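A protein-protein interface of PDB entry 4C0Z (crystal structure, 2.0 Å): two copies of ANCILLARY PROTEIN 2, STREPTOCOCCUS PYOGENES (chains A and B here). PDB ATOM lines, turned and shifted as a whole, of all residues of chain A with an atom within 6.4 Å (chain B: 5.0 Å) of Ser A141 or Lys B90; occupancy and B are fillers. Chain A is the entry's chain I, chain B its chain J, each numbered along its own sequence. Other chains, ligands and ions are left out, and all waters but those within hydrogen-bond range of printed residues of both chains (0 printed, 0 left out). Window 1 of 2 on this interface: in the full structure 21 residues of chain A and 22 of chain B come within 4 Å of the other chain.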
ATOM      1  N   LEU A  58      33.918 -10.308 -22.380  1.00  0.00           N
ATOM      2  CA  LEU A  58      34.218 -11.213 -21.271  1.00  0.00           C
ATOM      3  C   LEU A  58      35.460 -12.067 -21.448  1.00  0.00           C
ATOM      4  O   LEU A  58      36.024 -12.513 -20.455  1.00  0.00           O
ATOM      5  CB  LEU A  58      33.007 -12.111 -20.961  1.00  0.00           C
ATOM      6  CG  LEU A  58      31.799 -11.450 -20.329  1.00  0.00           C
ATOM      7  CD1 LEU A  58      30.670 -12.463 -20.184  1.00  0.00           C
ATOM      8  CD2 LEU A  58      32.156 -10.872 -18.976  1.00  0.00           C
ATOM      9  N   LYS A  90      29.831 -10.749 -28.662  1.00  0.00           N
ATOM     10  CA  LYS A  90      28.484 -11.342 -28.766  1.00  0.00           C
ATOM     11  C   LYS A  90      27.382 -10.382 -28.264  1.00  0.00           C
ATOM     12  O   LYS A  90      26.726 -10.710 -27.269  1.00  0.00           O
ATOM     13  CB  LYS A  90      28.421 -12.664 -27.952  1.00  0.00           C
ATOM     14  CG  LYS A  90      29.421 -13.738 -28.362  1.00  0.00           C
ATOM     15  CD  LYS A  90      29.684 -14.732 -27.234  1.00  0.00           C
ATOM     16  CE  LYS A  90      30.650 -15.794 -27.681  1.00  0.00           C
ATOM     17  NZ  LYS A  90      31.311 -16.444 -26.527  1.00  0.00           N
ATOM     18  N   ARG A  92      23.756  -8.670 -27.578  1.00  0.00           N
ATOM     19  CA  ARG A  92      22.356  -9.112 -27.596  1.00  0.00           C
ATOM     20  C   ARG A  92      21.579  -8.067 -28.415  1.00  0.00           C
ATOM     21  O   ARG A  92      21.035  -7.108 -27.856  1.00  0.00           O
ATOM     22  CB  ARG A  92      21.825  -9.242 -26.156  1.00  0.00           C
ATOM     23  CG  ARG A  92      20.610 -10.124 -26.022  1.00  0.00           C
ATOM     24  CD  ARG A  92      20.083 -10.188 -24.592  1.00  0.00           C
ATOM     25  NE  ARG A  92      20.957 -10.953 -23.695  1.00  0.00           N
ATOM     26  CZ  ARG A  92      20.917 -12.271 -23.525  1.00  0.00           C
ATOM     27  NH1 ARG A  92      20.044 -13.009 -24.200  1.00  0.00           N
ATOM     28  NH2 ARG A  92      21.750 -12.861 -22.682  1.00  0.00           N
ATOM     29  N   ASN A 132      26.700  -6.702 -14.208  1.00  0.00           N
ATOM     30  CA  ASN A 132      26.027  -7.930 -14.622  1.00  0.00           C
ATOM     31  C   ASN A 132      24.885  -7.664 -15.589  1.00  0.00           C
ATOM     32  O   ASN A 132      24.736  -8.411 -16.545  1.00  0.00           O
ATOM     33  CB  ASN A 132      25.601  -8.761 -13.420  1.00  0.00           C
ATOM     34  CG  ASN A 132      26.717  -9.696 -13.007  1.00  0.00           C
ATOM     35  OD1 ASN A 132      26.741 -10.841 -13.420  1.00  0.00           O
ATOM     36  ND2 ASN A 132      27.742  -9.204 -12.307  1.00  0.00           N
ATOM     37  N   ALA A 133      24.142  -6.558 -15.398  1.00  0.00           N
ATOM     38  CA  ALA A 133      23.076  -6.143 -16.310  1.00  0.00           C
ATOM     39  C   ALA A 133      23.689  -5.679 -17.658  1.00  0.00           C
ATOM     40  O   ALA A 133      23.172  -6.028 -18.721  1.00  0.00           O
ATOM     41  CB  ALA A 133      22.244  -5.039 -15.679  1.00  0.00           C
ATOM     42  N   ILE A 134      24.818  -4.956 -17.610  1.00  0.00           N
ATOM     43  CA  ILE A 134      25.564  -4.533 -18.806  1.00  0.00           C
ATOM     44  C   ILE A 134      26.036  -5.760 -19.632  1.00  0.00           C
ATOM     45  O   ILE A 134      25.766  -5.821 -20.839  1.00  0.00           O
ATOM     46  CB  ILE A 134      26.746  -3.577 -18.434  1.00  0.00           C
ATOM     47  CG1 ILE A 134      26.223  -2.163 -17.956  1.00  0.00           C
ATOM     48  CG2 ILE A 134      27.779  -3.457 -19.574  1.00  0.00           C
ATOM     49  CD1 ILE A 134      25.493  -1.305 -19.015  1.00  0.00           C
ATOM     50  N   TRP A 135      26.685  -6.739 -18.969  1.00  0.00           N
ATOM     51  CA  TRP A 135      27.185  -7.972 -19.602  1.00  0.00           C
ATOM     52  C   TRP A 135      26.086  -8.772 -20.265  1.00  0.00           C
ATOM     53  O   TRP A 135      26.347  -9.402 -21.289  1.00  0.00           O
ATOM     54  CB  TRP A 135      27.930  -8.865 -18.606  1.00  0.00           C
ATOM     55  CG  TRP A 135      29.290  -8.378 -18.233  1.00  0.00           C
ATOM     56  CD1 TRP A 135      30.164  -7.696 -19.024  1.00  0.00           C
ATOM     57  CD2 TRP A 135      29.994  -8.673 -17.020  1.00  0.00           C
ATOM     58  NE1 TRP A 135      31.338  -7.491 -18.355  1.00  0.00           N
ATOM     59  CE2 TRP A 135      31.263  -8.076 -17.121  1.00  0.00           C
ATOM     60  CE3 TRP A 135      29.660  -9.360 -15.844  1.00  0.00           C
ATOM     61  CZ2 TRP A 135      32.198  -8.138 -16.095  1.00  0.00           C
ATOM     62  CZ3 TRP A 135      30.580  -9.409 -14.824  1.00  0.00           C
ATOM     63  CH2 TRP A 135      31.843  -8.828 -14.960  1.00  0.00           C
ATOM     64  N   TYR A 136      24.861  -8.749 -19.689  1.00  0.00           N
ATOM     65  CA  TYR A 136      23.701  -9.424 -20.250  1.00  0.00           C
ATOM     66  C   TYR A 136      23.474  -8.919 -21.698  1.00  0.00           C
ATOM     67  O   TYR A 136      23.177  -9.713 -22.586  1.00  0.00           O
ATOM     68  CB  TYR A 136      22.456  -9.161 -19.364  1.00  0.00           C
ATOM     69  CG  TYR A 136      21.174  -9.756 -19.901  1.00  0.00           C
ATOM     70  CD1 TYR A 136      20.879 -11.104 -19.724  1.00  0.00           C
ATOM     71  CD2 TYR A 136      20.248  -8.970 -20.573  1.00  0.00           C
ATOM     72  CE1 TYR A 136      19.694 -11.654 -20.211  1.00  0.00           C
ATOM     73  CE2 TYR A 136      19.062  -9.510 -21.070  1.00  0.00           C
ATOM     74  CZ  TYR A 136      18.792 -10.853 -20.891  1.00  0.00           C
ATOM     75  OH  TYR A 136      17.638 -11.396 -21.390  1.00  0.00           O
ATOM     76  N   TYR A 137      23.651  -7.606 -21.932  1.00  0.00           N
ATOM     77  CA  TYR A 137      23.449  -7.022 -23.259  1.00  0.00           C
ATOM     78  C   TYR A 137      24.699  -7.016 -24.126  1.00  0.00           C
ATOM     79  O   TYR A 137      24.609  -7.352 -25.303  1.00  0.00           O
ATOM     80  CB  TYR A 137      22.843  -5.613 -23.159  1.00  0.00           C
ATOM     81  CG  TYR A 137      21.381  -5.646 -22.767  1.00  0.00           C
ATOM     82  CD1 TYR A 137      20.396  -5.974 -23.697  1.00  0.00           C
ATOM     83  CD2 TYR A 137      20.986  -5.413 -21.453  1.00  0.00           C
ATOM     84  CE1 TYR A 137      19.053  -6.056 -23.328  1.00  0.00           C
ATOM     85  CE2 TYR A 137      19.642  -5.463 -21.078  1.00  0.00           C
ATOM     86  CZ  TYR A 137      18.681  -5.786 -22.018  1.00  0.00           C
ATOM     87  OH  TYR A 137      17.371  -5.854 -21.621  1.00  0.00           O
ATOM     88  N   THR A 138      25.842  -6.629 -23.573  1.00  0.00           N
ATOM     89  CA  THR A 138      27.079  -6.510 -24.352  1.00  0.00           C
ATOM     90  C   THR A 138      27.714  -7.841 -24.757  1.00  0.00           C
ATOM     91  O   THR A 138      28.385  -7.912 -25.789  1.00  0.00           O
ATOM     92  CB  THR A 138      28.108  -5.690 -23.584  1.00  0.00           C
ATOM     93  OG1 THR A 138      28.468  -6.388 -22.394  1.00  0.00           O
ATOM     94  CG2 THR A 138      27.640  -4.280 -23.293  1.00  0.00           C
ATOM     95  N   ASP A 139      27.544  -8.873 -23.924  1.00  0.00           N
ATOM     96  CA  ASP A 139      28.181 -10.170 -24.130  1.00  0.00           C
ATOM     97  C   ASP A 139      27.209 -11.338 -24.141  1.00  0.00           C
ATOM     98  O   ASP A 139      27.651 -12.485 -24.140  1.00  0.00           O
ATOM     99  CB  ASP A 139      29.236 -10.366 -23.034  1.00  0.00           C
ATOM    100  CG  ASP A 139      30.472  -9.539 -23.269  1.00  0.00           C
ATOM    101  OD1 ASP A 139      30.496  -8.364 -22.825  1.00  0.00           O
ATOM    102  OD2 ASP A 139      31.385 -10.028 -23.972  1.00  0.00           O
ATOM    103  N   SER A 140      25.901 -11.055 -24.165  1.00  0.00           N
ATOM    104  CA  SER A 140      24.823 -12.055 -24.121  1.00  0.00           C
ATOM    105  C   SER A 140      25.052 -13.055 -22.966  1.00  0.00           C
ATOM    106  O   SER A 140      24.904 -14.269 -23.154  1.00  0.00           O
ATOM    107  CB  SER A 140      24.646 -12.756 -25.473  1.00  0.00           C
ATOM    108  OG  SER A 140      24.400 -11.828 -26.515  1.00  0.00           O
ATOM    109  N   SER A 141      25.474 -12.544 -21.782  1.00  0.00           N
ATOM    110  CA  SER A 141      25.712 -13.425 -20.641  1.00  0.00           C
ATOM    111  C   SER A 141      24.399 -14.031 -20.164  1.00  0.00           C
ATOM    112  O   SER A 141      23.364 -13.354 -20.148  1.00  0.00           O
ATOM    113  CB  SER A 141      26.478 -12.733 -19.524  1.00  0.00           C
ATOM    114  OG  SER A 141      25.640 -11.843 -18.811  1.00  0.00           O
ATOM    115  N   TYR A 142      24.426 -15.328 -19.873  1.00  0.00           N
ATOM    116  CA  TYR A 142      23.243 -16.095 -19.507  1.00  0.00           C
ATOM    117  C   TYR A 142      22.617 -15.703 -18.170  1.00  0.00           C
ATOM    118  O   TYR A 142      23.253 -15.815 -17.128  1.00  0.00           O
ATOM    119  CB  TYR A 142      23.558 -17.601 -19.545  1.00  0.00           C
ATOM    120  CG  TYR A 142      22.357 -18.503 -19.357  1.00  0.00           C
ATOM    121  CD1 TYR A 142      21.493 -18.778 -20.415  1.00  0.00           C
ATOM    122  CD2 TYR A 142      22.103 -19.112 -18.132  1.00  0.00           C
ATOM    123  CE1 TYR A 142      20.388 -19.616 -20.250  1.00  0.00           C
ATOM    124  CE2 TYR A 142      21.002 -19.951 -17.955  1.00  0.00           C
ATOM    125  CZ  TYR A 142      20.155 -20.209 -19.020  1.00  0.00           C
ATOM    126  OH  TYR A 142      19.081 -21.045 -18.845  1.00  0.00           O
ATOM    127  N   ILE A 143      21.370 -15.230 -18.209  1.00  0.00           N
ATOM    128  CA  ILE A 143      20.574 -14.920 -17.015  1.00  0.00           C
ATOM    129  C   ILE A 143      19.171 -15.467 -17.272  1.00  0.00           C
ATOM    130  O   ILE A 143      18.427 -14.890 -18.066  1.00  0.00           O
ATOM    131  CB  ILE A 143      20.551 -13.425 -16.570  1.00  0.00           C
ATOM    132  CG1 ILE A 143      21.959 -12.820 -16.411  1.00  0.00           C
ATOM    133  CG2 ILE A 143      19.740 -13.302 -15.275  1.00  0.00           C
ATOM    134  CD1 ILE A 143      22.039 -11.309 -16.191  1.00  0.00           C
ATOM    135  N   GLN A 152      28.112 -17.540  -6.677  1.00  0.00           N
ATOM    136  CA  GLN A 152      29.570 -17.514  -6.477  1.00  0.00           C
ATOM    137  C   GLN A 152      29.981 -16.284  -5.666  1.00  0.00           C
ATOM    138  O   GLN A 152      30.778 -16.410  -4.735  1.00  0.00           O
ATOM    139  CB  GLN A 152      30.344 -17.579  -7.816  1.00  0.00           C
ATOM    140  CG  GLN A 152      30.286 -18.939  -8.525  1.00  0.00           C
ATOM    141  CD  GLN A 152      30.852 -20.104  -7.740  1.00  0.00           C
ATOM    142  OE1 GLN A 152      31.987 -20.083  -7.256  1.00  0.00           O
ATOM    143  NE2 GLN A 152      30.068 -21.161  -7.635  1.00  0.00           N
ATOM    144  N   ALA B  88      31.465 -23.124 -10.654  1.00  0.00           N
ATOM    145  CA  ALA B  88      31.105 -22.377 -11.858  1.00  0.00           C
ATOM    146  C   ALA B  88      30.026 -21.362 -11.560  1.00  0.00           C
ATOM    147  O   ALA B  88      29.132 -21.605 -10.740  1.00  0.00           O
ATOM    148  CB  ALA B  88      30.660 -23.316 -12.965  1.00  0.00           C
ATOM    149  N   ASP B  89      30.117 -20.208 -12.229  1.00  0.00           N
ATOM    150  CA  ASP B  89      29.163 -19.112 -12.114  1.00  0.00           C
ATOM    151  C   ASP B  89      27.819 -19.486 -12.775  1.00  0.00           C
ATOM    152  O   ASP B  89      26.793 -19.489 -12.094  1.00  0.00           O
ATOM    153  CB  ASP B  89      29.738 -17.817 -12.739  1.00  0.00           C
ATOM    154  CG  ASP B  89      31.194 -17.462 -12.434  1.00  0.00           C
ATOM    155  OD1 ASP B  89      31.681 -17.806 -11.321  1.00  0.00           O
ATOM    156  OD2 ASP B  89      31.829 -16.773 -13.276  1.00  0.00           O
ATOM    157  N   LYS B  90      27.827 -19.807 -14.095  1.00  0.00           N
ATOM    158  CA  LYS B  90      26.629 -20.119 -14.877  1.00  0.00           C
ATOM    159  C   LYS B  90      26.813 -21.430 -15.681  1.00  0.00           C
ATOM    160  O   LYS B  90      26.843 -21.368 -16.910  1.00  0.00           O
ATOM    161  CB  LYS B  90      26.319 -18.958 -15.857  1.00  0.00           C
ATOM    162  CG  LYS B  90      26.068 -17.601 -15.233  1.00  0.00           C
ATOM    163  CD  LYS B  90      26.346 -16.471 -16.219  1.00  0.00           C
ATOM    164  CE  LYS B  90      26.171 -15.121 -15.567  1.00  0.00           C
ATOM    165  NZ  LYS B  90      26.894 -14.049 -16.302  1.00  0.00           N
ATOM    166  N   PRO B  91      26.942 -22.622 -15.060  1.00  0.00           N
ATOM    167  CA  PRO B  91      27.105 -23.841 -15.878  1.00  0.00           C
ATOM    168  C   PRO B  91      25.849 -24.228 -16.667  1.00  0.00           C
ATOM    169  O   PRO B  91      24.730 -24.012 -16.206  1.00  0.00           O
ATOM    170  CB  PRO B  91      27.494 -24.899 -14.854  1.00  0.00           C
ATOM    171  CG  PRO B  91      26.848 -24.442 -13.580  1.00  0.00           C
ATOM    172  CD  PRO B  91      26.924 -22.935 -13.616  1.00  0.00           C
ATOM    173  N   ARG B  92      26.036 -24.780 -17.873  1.00  0.00           N
ATOM    174  CA  ARG B  92      24.932 -25.214 -18.726  1.00  0.00           C
ATOM    175  C   ARG B  92      24.590 -26.660 -18.286  1.00  0.00           C
ATOM    176  O   ARG B  92      25.136 -27.634 -18.818  1.00  0.00           O
ATOM    177  CB  ARG B  92      25.360 -25.126 -20.200  1.00  0.00           C
ATOM    178  CG  ARG B  92      24.199 -25.154 -21.179  1.00  0.00           C
ATOM    179  CD  ARG B  92      24.669 -25.139 -22.621  1.00  0.00           C
ATOM    180  NE  ARG B  92      25.270 -23.860 -23.013  1.00  0.00           N
ATOM    181  CZ  ARG B  92      24.589 -22.812 -23.467  1.00  0.00           C
ATOM    182  NH1 ARG B  92      23.268 -22.866 -23.579  1.00  0.00           N
ATOM    183  NH2 ARG B  92      25.224 -21.697 -23.804  1.00  0.00           N
ATOM    184  N   TYR B 137      29.774 -24.652 -22.195  1.00  0.00           N
ATOM    185  CA  TYR B 137      29.237 -25.460 -21.108  1.00  0.00           C
ATOM    186  C   TYR B 137      29.499 -24.897 -19.724  1.00  0.00           C
ATOM    187  O   TYR B 137      28.594 -24.899 -18.895  1.00  0.00           O
ATOM    188  CB  TYR B 137      29.717 -26.911 -21.202  1.00  0.00           C
ATOM    189  CG  TYR B 137      29.034 -27.663 -22.320  1.00  0.00           C
ATOM    190  CD1 TYR B 137      27.733 -28.144 -22.174  1.00  0.00           C
ATOM    191  CD2 TYR B 137      29.668 -27.865 -23.538  1.00  0.00           C
ATOM    192  CE1 TYR B 137      27.078 -28.795 -23.222  1.00  0.00           C
ATOM    193  CE2 TYR B 137      29.037 -28.545 -24.581  1.00  0.00           C
ATOM    194  CZ  TYR B 137      27.740 -29.007 -24.422  1.00  0.00           C
ATOM    195  OH  TYR B 137      27.114 -29.657 -25.465  1.00  0.00           O
ATOM    196  N   THR B 138      30.723 -24.430 -19.455  1.00  0.00           N
ATOM    197  CA  THR B 138      31.075 -23.949 -18.118  1.00  0.00           C
ATOM    198  C   THR B 138      30.461 -22.626 -17.740  1.00  0.00           C
ATOM    199  O   THR B 138      30.238 -22.376 -16.551  1.00  0.00           O
ATOM    200  CB  THR B 138      32.592 -23.875 -17.964  1.00  0.00           C
ATOM    201  OG1 THR B 138      33.133 -22.882 -18.880  1.00  0.00           O
ATOM    202  CG2 THR B 138      33.272 -25.231 -18.137  1.00  0.00           C
ATOM    203  N   ASP B 139      30.244 -21.754 -18.731  1.00  0.00           N
ATOM    204  CA  ASP B 139      29.784 -20.404 -18.493  1.00  0.00           C
ATOM    205  C   ASP B 139      28.552 -20.029 -19.281  1.00  0.00           C
ATOM    206  O   ASP B 139      28.195 -18.849 -19.305  1.00  0.00           O
ATOM    207  CB  ASP B 139      30.934 -19.433 -18.820  1.00  0.00           C
ATOM    208  CG  ASP B 139      32.036 -19.430 -17.787  1.00  0.00           C
ATOM    209  OD1 ASP B 139      32.934 -20.299 -17.876  1.00  0.00           O
ATOM    210  OD2 ASP B 139      32.013 -18.561 -16.906  1.00  0.00           O
ATOM    211  N   SER B 140      27.896 -21.020 -19.922  1.00  0.00           N
ATOM    212  CA  SER B 140      26.725 -20.822 -20.766  1.00  0.00           C
ATOM    213  C   SER B 140      26.950 -19.702 -21.769  1.00  0.00           C
ATOM    214  O   SER B 140      26.074 -18.860 -21.956  1.00  0.00           O
ATOM    215  CB  SER B 140      25.457 -20.606 -19.938  1.00  0.00           C
ATOM    216  OG  SER B 140      25.235 -21.678 -19.039  1.00  0.00           O
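O of Ala B88 sits at hydrogen-bond distance from NE2 of Gln A152.
Of chain B, only Lys B90 comes within 4 Å of Ser A141. Lys B90 touches just these residues of chain A: Ser A141 and Tyr A142. Printed residues of chain A within 4 Å of Asp B89: Gln A152. Of the printed residues of chain B, Gln A152 touches Ala B88 (3.3 Å) and Asp B89 (3.3 Å). Printed residues of chain B within 4 Å of Tyr A142: Lys B90 and Ser B140. Printed residues of chain A within 4 Å of Ser B140: Tyr A142 (3.6 Å). Printed residues of chain A within 4 Å of Ala B88: Gln A152 (3.3 Å). Leu A58 touches none of the printed residues of chain B. Ile A134 touches none of the printed residues of chain B. The nearest printed residue of chain A that does not touch Asp B89 is Tyr A142 (7.2 Å).
CB of Ser A141 touches NZ of Lys B90 (3.5 Å). Tyr A142 touches Lys B90 (O to CD, 3.3 Å). Ser B140 touches Tyr A142. Asp B89 touches Gln A152.
The guanidinium group (NH2) of Arg A92 lies within hydrogen-bond range of the backbone carbonyl oxygen (O) of Ser A141, 3.0 Å away. N of Ser A141 lies within hydrogen-bond range of O of Trp A135, 3.3 Å away. The side-chain hydroxyl of Ser A141 sits at hydrogen-bond distance from the backbone NH of Tyr A136 (3.3 Å). The backbone carbonyl oxygen of Lys B90 lies within hydrogen-bond range of the side-chain hydroxyl of Ser B140 (2.7 Å). The backbone NH (N) of Arg B92 lies within hydrogen-bond range of the side-chain hydroxyl (OG) of Ser B140 (3.4 Å).
Positions printed for both chains: 90, 92, 137, 138, 139 and 140.
Of the 16 printed residues of chain A, 3 touch a printed residue of chain B. Hydrophobic or aromatic side chains of chain A within 4 Å of the printed part of chain B: Tyr A142. Among the printed residues, 5 pairs touch across the chains. Among the printed residues, no Asp or Glu carboxylate lies within 4 Å of a Lys or Arg side-chain nitrogen of the other chain.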
